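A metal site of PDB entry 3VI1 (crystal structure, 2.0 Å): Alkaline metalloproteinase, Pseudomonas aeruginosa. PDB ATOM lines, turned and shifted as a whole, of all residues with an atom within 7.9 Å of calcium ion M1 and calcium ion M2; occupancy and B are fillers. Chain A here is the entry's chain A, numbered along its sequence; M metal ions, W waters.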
ATOM      1  N   THR A 252     -21.314 -20.110 -10.333  1.00  0.00           N
ATOM      2  CA  THR A 252     -22.557 -20.878 -10.351  1.00  0.00           C
ATOM      3  C   THR A 252     -22.752 -21.717  -9.084  1.00  0.00           C
ATOM      4  O   THR A 252     -21.922 -22.558  -8.758  1.00  0.00           O
ATOM      5  CB  THR A 252     -22.646 -21.768 -11.606  1.00  0.00           C
ATOM      6  OG1 THR A 252     -22.428 -20.970 -12.779  1.00  0.00           O
ATOM      7  CG2 THR A 252     -24.000 -22.440 -11.713  1.00  0.00           C
ATOM      8  N   ARG A 253     -23.874 -21.484  -8.403  1.00  0.00           N
ATOM      9  CA  ARG A 253     -24.257 -22.224  -7.200  1.00  0.00           C
ATOM     10  C   ARG A 253     -23.107 -22.347  -6.196  1.00  0.00           C
ATOM     11  O   ARG A 253     -22.701 -23.453  -5.835  1.00  0.00           O
ATOM     12  CB  ARG A 253     -24.809 -23.605  -7.581  1.00  0.00           C
ATOM     13  CG  ARG A 253     -26.099 -23.572  -8.392  1.00  0.00           C
ATOM     14  CD  ARG A 253     -26.526 -24.966  -8.835  1.00  0.00           C
ATOM     15  NE  ARG A 253     -25.689 -25.480  -9.921  1.00  0.00           N
ATOM     16  CZ  ARG A 253     -25.974 -25.372 -11.212  1.00  0.00           C
ATOM     17  NH1 ARG A 253     -27.081 -24.759 -11.610  1.00  0.00           N
ATOM     18  NH2 ARG A 253     -25.147 -25.885 -12.115  1.00  0.00           N
ATOM     19  N   THR A 254     -22.594 -21.200  -5.766  1.00  0.00           N
ATOM     20  CA  THR A 254     -21.460 -21.152  -4.837  1.00  0.00           C
ATOM     21  C   THR A 254     -21.867 -21.409  -3.385  1.00  0.00           C
ATOM     22  O   THR A 254     -21.017 -21.689  -2.533  1.00  0.00           O
ATOM     23  CB  THR A 254     -20.690 -19.815  -4.929  1.00  0.00           C
ATOM     24  OG1 THR A 254     -21.593 -18.723  -4.776  1.00  0.00           O
ATOM     25  CG2 THR A 254     -19.986 -19.701  -6.277  1.00  0.00           C
ATOM     26  N   GLY A 255     -23.168 -21.302  -3.097  1.00  0.00           N
ATOM     27  CA  GLY A 255     -23.699 -21.575  -1.775  1.00  0.00           C
ATOM     28  C   GLY A 255     -24.017 -23.050  -1.579  1.00  0.00           C
ATOM     29  O   GLY A 255     -23.680 -23.875  -2.430  1.00  0.00           O
ATOM     30  N   ASP A 256     -24.654 -23.377  -0.454  1.00  0.00           N
ATOM     31  CA  ASP A 256     -25.038 -24.745  -0.144  1.00  0.00           C
ATOM     32  C   ASP A 256     -26.168 -25.208  -1.061  1.00  0.00           C
ATOM     33  O   ASP A 256     -27.278 -24.670  -1.003  1.00  0.00           O
ATOM     34  CB  ASP A 256     -25.426 -24.879   1.330  1.00  0.00           C
ATOM     35  CG  ASP A 256     -24.221 -24.837   2.274  1.00  0.00           C
ATOM     36  OD1 ASP A 256     -23.116 -24.476   1.816  1.00  0.00           O
ATOM     37  OD2 ASP A 256     -24.397 -25.157   3.467  1.00  0.00           O
ATOM     38  N   THR A 257     -25.875 -26.192  -1.905  1.00  0.00           N
ATOM     39  CA  THR A 257     -26.791 -26.622  -2.950  1.00  0.00           C
ATOM     40  C   THR A 257     -27.236 -28.071  -2.778  1.00  0.00           C
ATOM     41  O   THR A 257     -26.413 -28.972  -2.599  1.00  0.00           O
ATOM     42  CB  THR A 257     -26.158 -26.456  -4.356  1.00  0.00           C
ATOM     43  OG1 THR A 257     -25.370 -25.274  -4.399  1.00  0.00           O
ATOM     44  CG2 THR A 257     -27.244 -26.383  -5.423  1.00  0.00           C
ATOM     45  N   VAL A 258     -28.546 -28.283  -2.827  1.00  0.00           N
ATOM     46  CA  VAL A 258     -29.114 -29.619  -2.725  1.00  0.00           C
ATOM     47  C   VAL A 258     -29.624 -30.082  -4.094  1.00  0.00           C
ATOM     48  O   VAL A 258     -30.396 -29.372  -4.747  1.00  0.00           O
ATOM     49  CB  VAL A 258     -30.254 -29.691  -1.666  1.00  0.00           C
ATOM     50  CG1 VAL A 258     -30.792 -31.114  -1.539  1.00  0.00           C
ATOM     51  CG2 VAL A 258     -29.747 -29.201  -0.313  1.00  0.00           C
ATOM     52  N   TYR A 259     -29.168 -31.250  -4.517  1.00  0.00           N
ATOM     53  CA  TYR A 259     -29.568 -31.842  -5.786  1.00  0.00           C
ATOM     54  C   TYR A 259     -30.466 -33.048  -5.554  1.00  0.00           C
ATOM     55  O   TYR A 259     -30.305 -33.774  -4.576  1.00  0.00           O
ATOM     56  CB  TYR A 259     -28.332 -32.246  -6.599  1.00  0.00           C
ATOM     57  CG  TYR A 259     -27.434 -31.085  -6.967  1.00  0.00           C
ATOM     58  CD1 TYR A 259     -26.452 -30.631  -6.084  1.00  0.00           C
ATOM     59  CD2 TYR A 259     -27.565 -30.450  -8.200  1.00  0.00           C
ATOM     60  CE1 TYR A 259     -25.631 -29.551  -6.420  1.00  0.00           C
ATOM     61  CE2 TYR A 259     -26.738 -29.378  -8.546  1.00  0.00           C
ATOM     62  CZ  TYR A 259     -25.774 -28.942  -7.646  1.00  0.00           C
ATOM     63  OH  TYR A 259     -24.970 -27.889  -7.988  1.00  0.00           O
ATOM     64  N   ASN A 264     -32.721 -26.777  -4.294  1.00  0.00           N
ATOM     65  CA  ASN A 264     -32.719 -25.313  -4.326  1.00  0.00           C
ATOM     66  C   ASN A 264     -32.006 -24.763  -5.562  1.00  0.00           C
ATOM     67  O   ASN A 264     -31.666 -23.576  -5.624  1.00  0.00           O
ATOM     68  CB  ASN A 264     -32.086 -24.751  -3.041  1.00  0.00           C
ATOM     69  CG  ASN A 264     -30.593 -25.082  -2.926  1.00  0.00           C
ATOM     70  OD1 ASN A 264     -30.134 -26.121  -3.414  1.00  0.00           O
ATOM     71  ND2 ASN A 264     -29.852 -24.199  -2.277  1.00  0.00           N
ATOM     72  N   VAL A 283     -23.616 -32.952 -12.304  1.00  0.00           N
ATOM     73  CA  VAL A 283     -23.517 -31.822 -11.372  1.00  0.00           C
ATOM     74  C   VAL A 283     -22.328 -30.909 -11.689  1.00  0.00           C
ATOM     75  O   VAL A 283     -21.176 -31.333 -11.588  1.00  0.00           O
ATOM     76  CB  VAL A 283     -23.390 -32.300  -9.900  1.00  0.00           C
ATOM     77  CG1 VAL A 283     -23.286 -31.118  -8.951  1.00  0.00           C
ATOM     78  CG2 VAL A 283     -24.557 -33.193  -9.517  1.00  0.00           C
ATOM     79  N   TRP A 284     -22.617 -29.677 -12.080  1.00  0.00           N
ATOM     80  CA  TRP A 284     -21.613 -28.618 -12.062  1.00  0.00           C
ATOM     81  C   TRP A 284     -21.882 -27.698 -10.883  1.00  0.00           C
ATOM     82  O   TRP A 284     -22.975 -27.138 -10.742  1.00  0.00           O
ATOM     83  CB  TRP A 284     -21.561 -27.818 -13.364  1.00  0.00           C
ATOM     84  CG  TRP A 284     -20.661 -26.619 -13.232  1.00  0.00           C
ATOM     85  CD1 TRP A 284     -21.040 -25.310 -13.170  1.00  0.00           C
ATOM     86  CD2 TRP A 284     -19.229 -26.626 -13.097  1.00  0.00           C
ATOM     87  NE1 TRP A 284     -19.945 -24.497 -13.028  1.00  0.00           N
ATOM     88  CE2 TRP A 284     -18.816 -25.275 -12.978  1.00  0.00           C
ATOM     89  CE3 TRP A 284     -18.257 -27.632 -13.070  1.00  0.00           C
ATOM     90  CZ2 TRP A 284     -17.472 -24.912 -12.829  1.00  0.00           C
ATOM     91  CZ3 TRP A 284     -16.927 -27.269 -12.931  1.00  0.00           C
ATOM     92  CH2 TRP A 284     -16.546 -25.921 -12.805  1.00  0.00           C
ATOM     93  N   ASP A 285     -20.872 -27.550 -10.023  1.00  0.00           N
ATOM     94  CA  ASP A 285     -21.022 -26.801  -8.785  1.00  0.00           C
ATOM     95  C   ASP A 285     -19.702 -26.135  -8.399  1.00  0.00           C
ATOM     96  O   ASP A 285     -18.669 -26.804  -8.305  1.00  0.00           O
ATOM     97  CB  ASP A 285     -21.495 -27.741  -7.667  1.00  0.00           C
ATOM     98  CG  ASP A 285     -22.042 -27.004  -6.477  1.00  0.00           C
ATOM     99  OD1 ASP A 285     -21.280 -26.266  -5.827  1.00  0.00           O
ATOM    100  OD2 ASP A 285     -23.248 -27.171  -6.173  1.00  0.00           O
ATOM    101  N   ALA A 286     -19.750 -24.822  -8.182  1.00  0.00           N
ATOM    102  CA  ALA A 286     -18.542 -24.015  -7.981  1.00  0.00           C
ATOM    103  C   ALA A 286     -18.009 -23.991  -6.545  1.00  0.00           C
ATOM    104  O   ALA A 286     -16.810 -23.784  -6.345  1.00  0.00           O
ATOM    105  CB  ALA A 286     -18.780 -22.593  -8.477  1.00  0.00           C
ATOM    106  N   GLY A 287     -18.878 -24.165  -5.560  1.00  0.00           N
ATOM    107  CA  GLY A 287     -18.457 -24.126  -4.161  1.00  0.00           C
ATOM    108  C   GLY A 287     -19.566 -24.370  -3.144  1.00  0.00           C
ATOM    109  O   GLY A 287     -20.731 -24.550  -3.507  1.00  0.00           O
ATOM    110  N   GLY A 288     -19.181 -24.370  -1.865  1.00  0.00           N
ATOM    111  CA  GLY A 288     -20.129 -24.559  -0.775  1.00  0.00           C
ATOM    112  C   GLY A 288     -20.288 -26.003  -0.350  1.00  0.00           C
ATOM    113  O   GLY A 288     -19.639 -26.907  -0.907  1.00  0.00           O
ATOM    114  N   ASN A 289     -21.143 -26.229   0.639  1.00  0.00           N
ATOM    115  CA  ASN A 289     -21.439 -27.560   1.164  1.00  0.00           C
ATOM    116  C   ASN A 289     -22.647 -28.149   0.445  1.00  0.00           C
ATOM    117  O   ASN A 289     -23.772 -27.681   0.623  1.00  0.00           O
ATOM    118  CB  ASN A 289     -21.691 -27.476   2.671  1.00  0.00           C
ATOM    119  CG  ASN A 289     -21.710 -28.835   3.339  1.00  0.00           C
ATOM    120  OD1 ASN A 289     -20.704 -29.555   3.339  1.00  0.00           O
ATOM    121  ND2 ASN A 289     -22.846 -29.185   3.927  1.00  0.00           N
ATOM    122  N   ASP A 290     -22.419 -29.177  -0.352  1.00  0.00           N
ATOM    123  CA  ASP A 290     -23.437 -29.655  -1.286  1.00  0.00           C
ATOM    124  C   ASP A 290     -23.916 -31.075  -1.023  1.00  0.00           C
ATOM    125  O   ASP A 290     -23.156 -31.927  -0.549  1.00  0.00           O
ATOM    126  CB  ASP A 290     -22.931 -29.514  -2.720  1.00  0.00           C
ATOM    127  CG  ASP A 290     -22.414 -28.116  -3.014  1.00  0.00           C
ATOM    128  OD1 ASP A 290     -23.168 -27.141  -2.803  1.00  0.00           O
ATOM    129  OD2 ASP A 290     -21.245 -27.987  -3.439  1.00  0.00           O
ATOM    130  N   THR A 291     -25.194 -31.319  -1.318  1.00  0.00           N
ATOM    131  CA  THR A 291     -25.846 -32.576  -0.982  1.00  0.00           C
ATOM    132  C   THR A 291     -26.596 -33.204  -2.156  1.00  0.00           C
ATOM    133  O   THR A 291     -27.368 -32.534  -2.845  1.00  0.00           O
ATOM    134  CB  THR A 291     -26.825 -32.392   0.205  1.00  0.00           C
ATOM    135  OG1 THR A 291     -26.153 -31.758   1.297  1.00  0.00           O
ATOM    136  CG2 THR A 291     -27.387 -33.729   0.677  1.00  0.00           C
ATOM    137  N   VAL A 326     -15.443 -30.793  -9.594  1.00  0.00           N
ATOM    138  CA  VAL A 326     -16.546 -30.500  -8.686  1.00  0.00           C
ATOM    139  C   VAL A 326     -16.450 -31.341  -7.408  1.00  0.00           C
ATOM    140  O   VAL A 326     -16.280 -32.557  -7.477  1.00  0.00           O
ATOM    141  CB  VAL A 326     -17.924 -30.726  -9.348  1.00  0.00           C
ATOM    142  CG1 VAL A 326     -19.065 -30.456  -8.367  1.00  0.00           C
ATOM    143  CG2 VAL A 326     -18.073 -29.866 -10.580  1.00  0.00           C
ATOM    144  N   THR A 327     -16.554 -30.679  -6.261  1.00  0.00           N
ATOM    145  CA  THR A 327     -16.556 -31.350  -4.967  1.00  0.00           C
ATOM    146  C   THR A 327     -17.959 -31.323  -4.350  1.00  0.00           C
ATOM    147  O   THR A 327     -18.461 -30.263  -3.969  1.00  0.00           O
ATOM    148  CB  THR A 327     -15.519 -30.740  -3.988  1.00  0.00           C
ATOM    149  OG1 THR A 327     -14.246 -30.650  -4.642  1.00  0.00           O
ATOM    150  CG2 THR A 327     -15.382 -31.596  -2.735  1.00  0.00           C
ATOM    151  N   VAL A 328     -18.581 -32.499  -4.280  1.00  0.00           N
ATOM    152  CA  VAL A 328     -19.873 -32.672  -3.613  1.00  0.00           C
ATOM    153  C   VAL A 328     -19.633 -33.356  -2.262  1.00  0.00           C
ATOM    154  O   VAL A 328     -18.952 -34.375  -2.190  1.00  0.00           O
ATOM    155  CB  VAL A 328     -20.871 -33.501  -4.470  1.00  0.00           C
ATOM    156  CG1 VAL A 328     -22.230 -33.605  -3.778  1.00  0.00           C
ATOM    157  CG2 VAL A 328     -21.027 -32.887  -5.853  1.00  0.00           C
ATOM    158  N   GLU A 329     -20.185 -32.769  -1.207  1.00  0.00           N
ATOM    159  CA  GLU A 329     -19.866 -33.189   0.153  1.00  0.00           C
ATOM    160  C   GLU A 329     -20.761 -34.292   0.710  1.00  0.00           C
ATOM    161  O   GLU A 329     -20.271 -35.233   1.332  1.00  0.00           O
ATOM    162  CB  GLU A 329     -19.899 -31.984   1.107  1.00  0.00           C
ATOM    163  CG  GLU A 329     -18.704 -31.036   0.971  1.00  0.00           C
ATOM    164  CD  GLU A 329     -18.704 -30.243  -0.323  1.00  0.00           C
ATOM    165  OE1 GLU A 329     -19.788 -29.983  -0.893  1.00  0.00           O
ATOM    166  OE2 GLU A 329     -17.608 -29.846  -0.788  1.00  0.00           O
ATOM    167  N   ASN A 330     -22.068 -34.180   0.497  1.00  0.00           N
ATOM    168  CA  ASN A 330     -23.035 -35.022   1.199  1.00  0.00           C
ATOM    169  C   ASN A 330     -23.926 -35.862   0.287  1.00  0.00           C
ATOM    170  O   ASN A 330     -24.217 -35.469  -0.843  1.00  0.00           O
ATOM    171  CB  ASN A 330     -23.891 -34.172   2.138  1.00  0.00           C
ATOM    172  CG  ASN A 330     -23.082 -33.128   2.886  1.00  0.00           C
ATOM    173  OD1 ASN A 330     -22.041 -33.418   3.468  1.00  0.00           O
ATOM    174  ND2 ASN A 330     -23.578 -31.885   2.879  1.00  0.00           N
ATOM    175  N   VAL A 345     -12.760 -35.584   0.836  1.00  0.00           N
ATOM    176  CA  VAL A 345     -13.049 -34.604   1.895  1.00  0.00           C
ATOM    177  C   VAL A 345     -14.059 -35.145   2.921  1.00  0.00           C
ATOM    178  O   VAL A 345     -14.525 -36.282   2.802  1.00  0.00           O
ATOM    179  CB  VAL A 345     -13.541 -33.236   1.313  1.00  0.00           C
ATOM    180  CG1 VAL A 345     -12.493 -32.621   0.398  1.00  0.00           C
ATOM    181  CG2 VAL A 345     -14.883 -33.372   0.598  1.00  0.00           C
HETATM  182 CA    CA M   1     -22.807 -25.155  -4.268  1.00  0.00          CA
HETATM  183 CA    CA M   2     -19.015 -28.340  -2.703  1.00  0.00          CA
HETATM  184  O   HOH W   1     -16.797 -27.503  -2.570  1.00  0.00           O
HETATM  185  O   HOH W   2     -19.062 -27.335  -4.850  1.00  0.00           O
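OD2 of Asp 285 sits close to OH of Tyr 259, 2.6 Å away.
The backbone NH (N) of Asn 330 sits at hydrogen-bond distance from the backbone carbonyl oxygen (O) of Asp 290, at 2.7 Å.
O of Trp 284 lies within hydrogen-bond range of NH2 of Arg 253, 2.9 Å away.
NE of Arg 253 is in hydrogen-bond range of OH of Tyr 259 (3.2 Å).
O of Thr 257 is in hydrogen-bond range of N of Thr 291, at 2.9 Å.
The backbone carbonyl oxygen (O) of Thr 254 lies within hydrogen-bond range of the backbone NH (N) of Gly 288 (3.3 Å).
Thr 254 touches calcium ion M1 (C to CA, 3.96 Å).
Within 4 Å of calcium ion M1: Arg 253, Thr 254, Gly 255, Thr 257, Asp 285, Gly 287 and Asp 290.
Within 4 Å of calcium ion M2: Gly 288, Asp 290, Thr 327 and Glu 329.
The nearest printed residue that does not touch calcium ion M2 is Gly 287 (4.03 Å).
O of Gly 287 binds calcium ion M1, 2.3 Å away.
Calcium ion M1 is bound by O of Arg 253 (2.3 Å).
O of Gly 255 is bound to calcium ion M1 (2.4 Å).
Calcium ion M1 is bound by OD1 of Asp 285 (2.4 Å).
Calcium ion M1 is bound by OD1 of Asp 290 (2.5 Å).
Calcium ion M1 is bound by OG1 of Thr 257 (2.6 Å).
The side-chain carboxylate (OD2) of Asp 285 is bound to calcium ion M1 (2.8 Å).
Calcium ion M1 has seven donor atoms within binding distance.
Calcium ion M2 is bound by the backbone carbonyl oxygen (O) of Thr 327, water W2, water W1, the side-chain carboxylate (OD2) of Asp 290, the backbone carbonyl oxygen (O) of Gly 288, the side-chain carboxylate (OE1) of Glu 329 and the side-chain carboxylate (OE2) of Glu 329.
Calcium ion M2 has seven donor atoms within binding distance.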
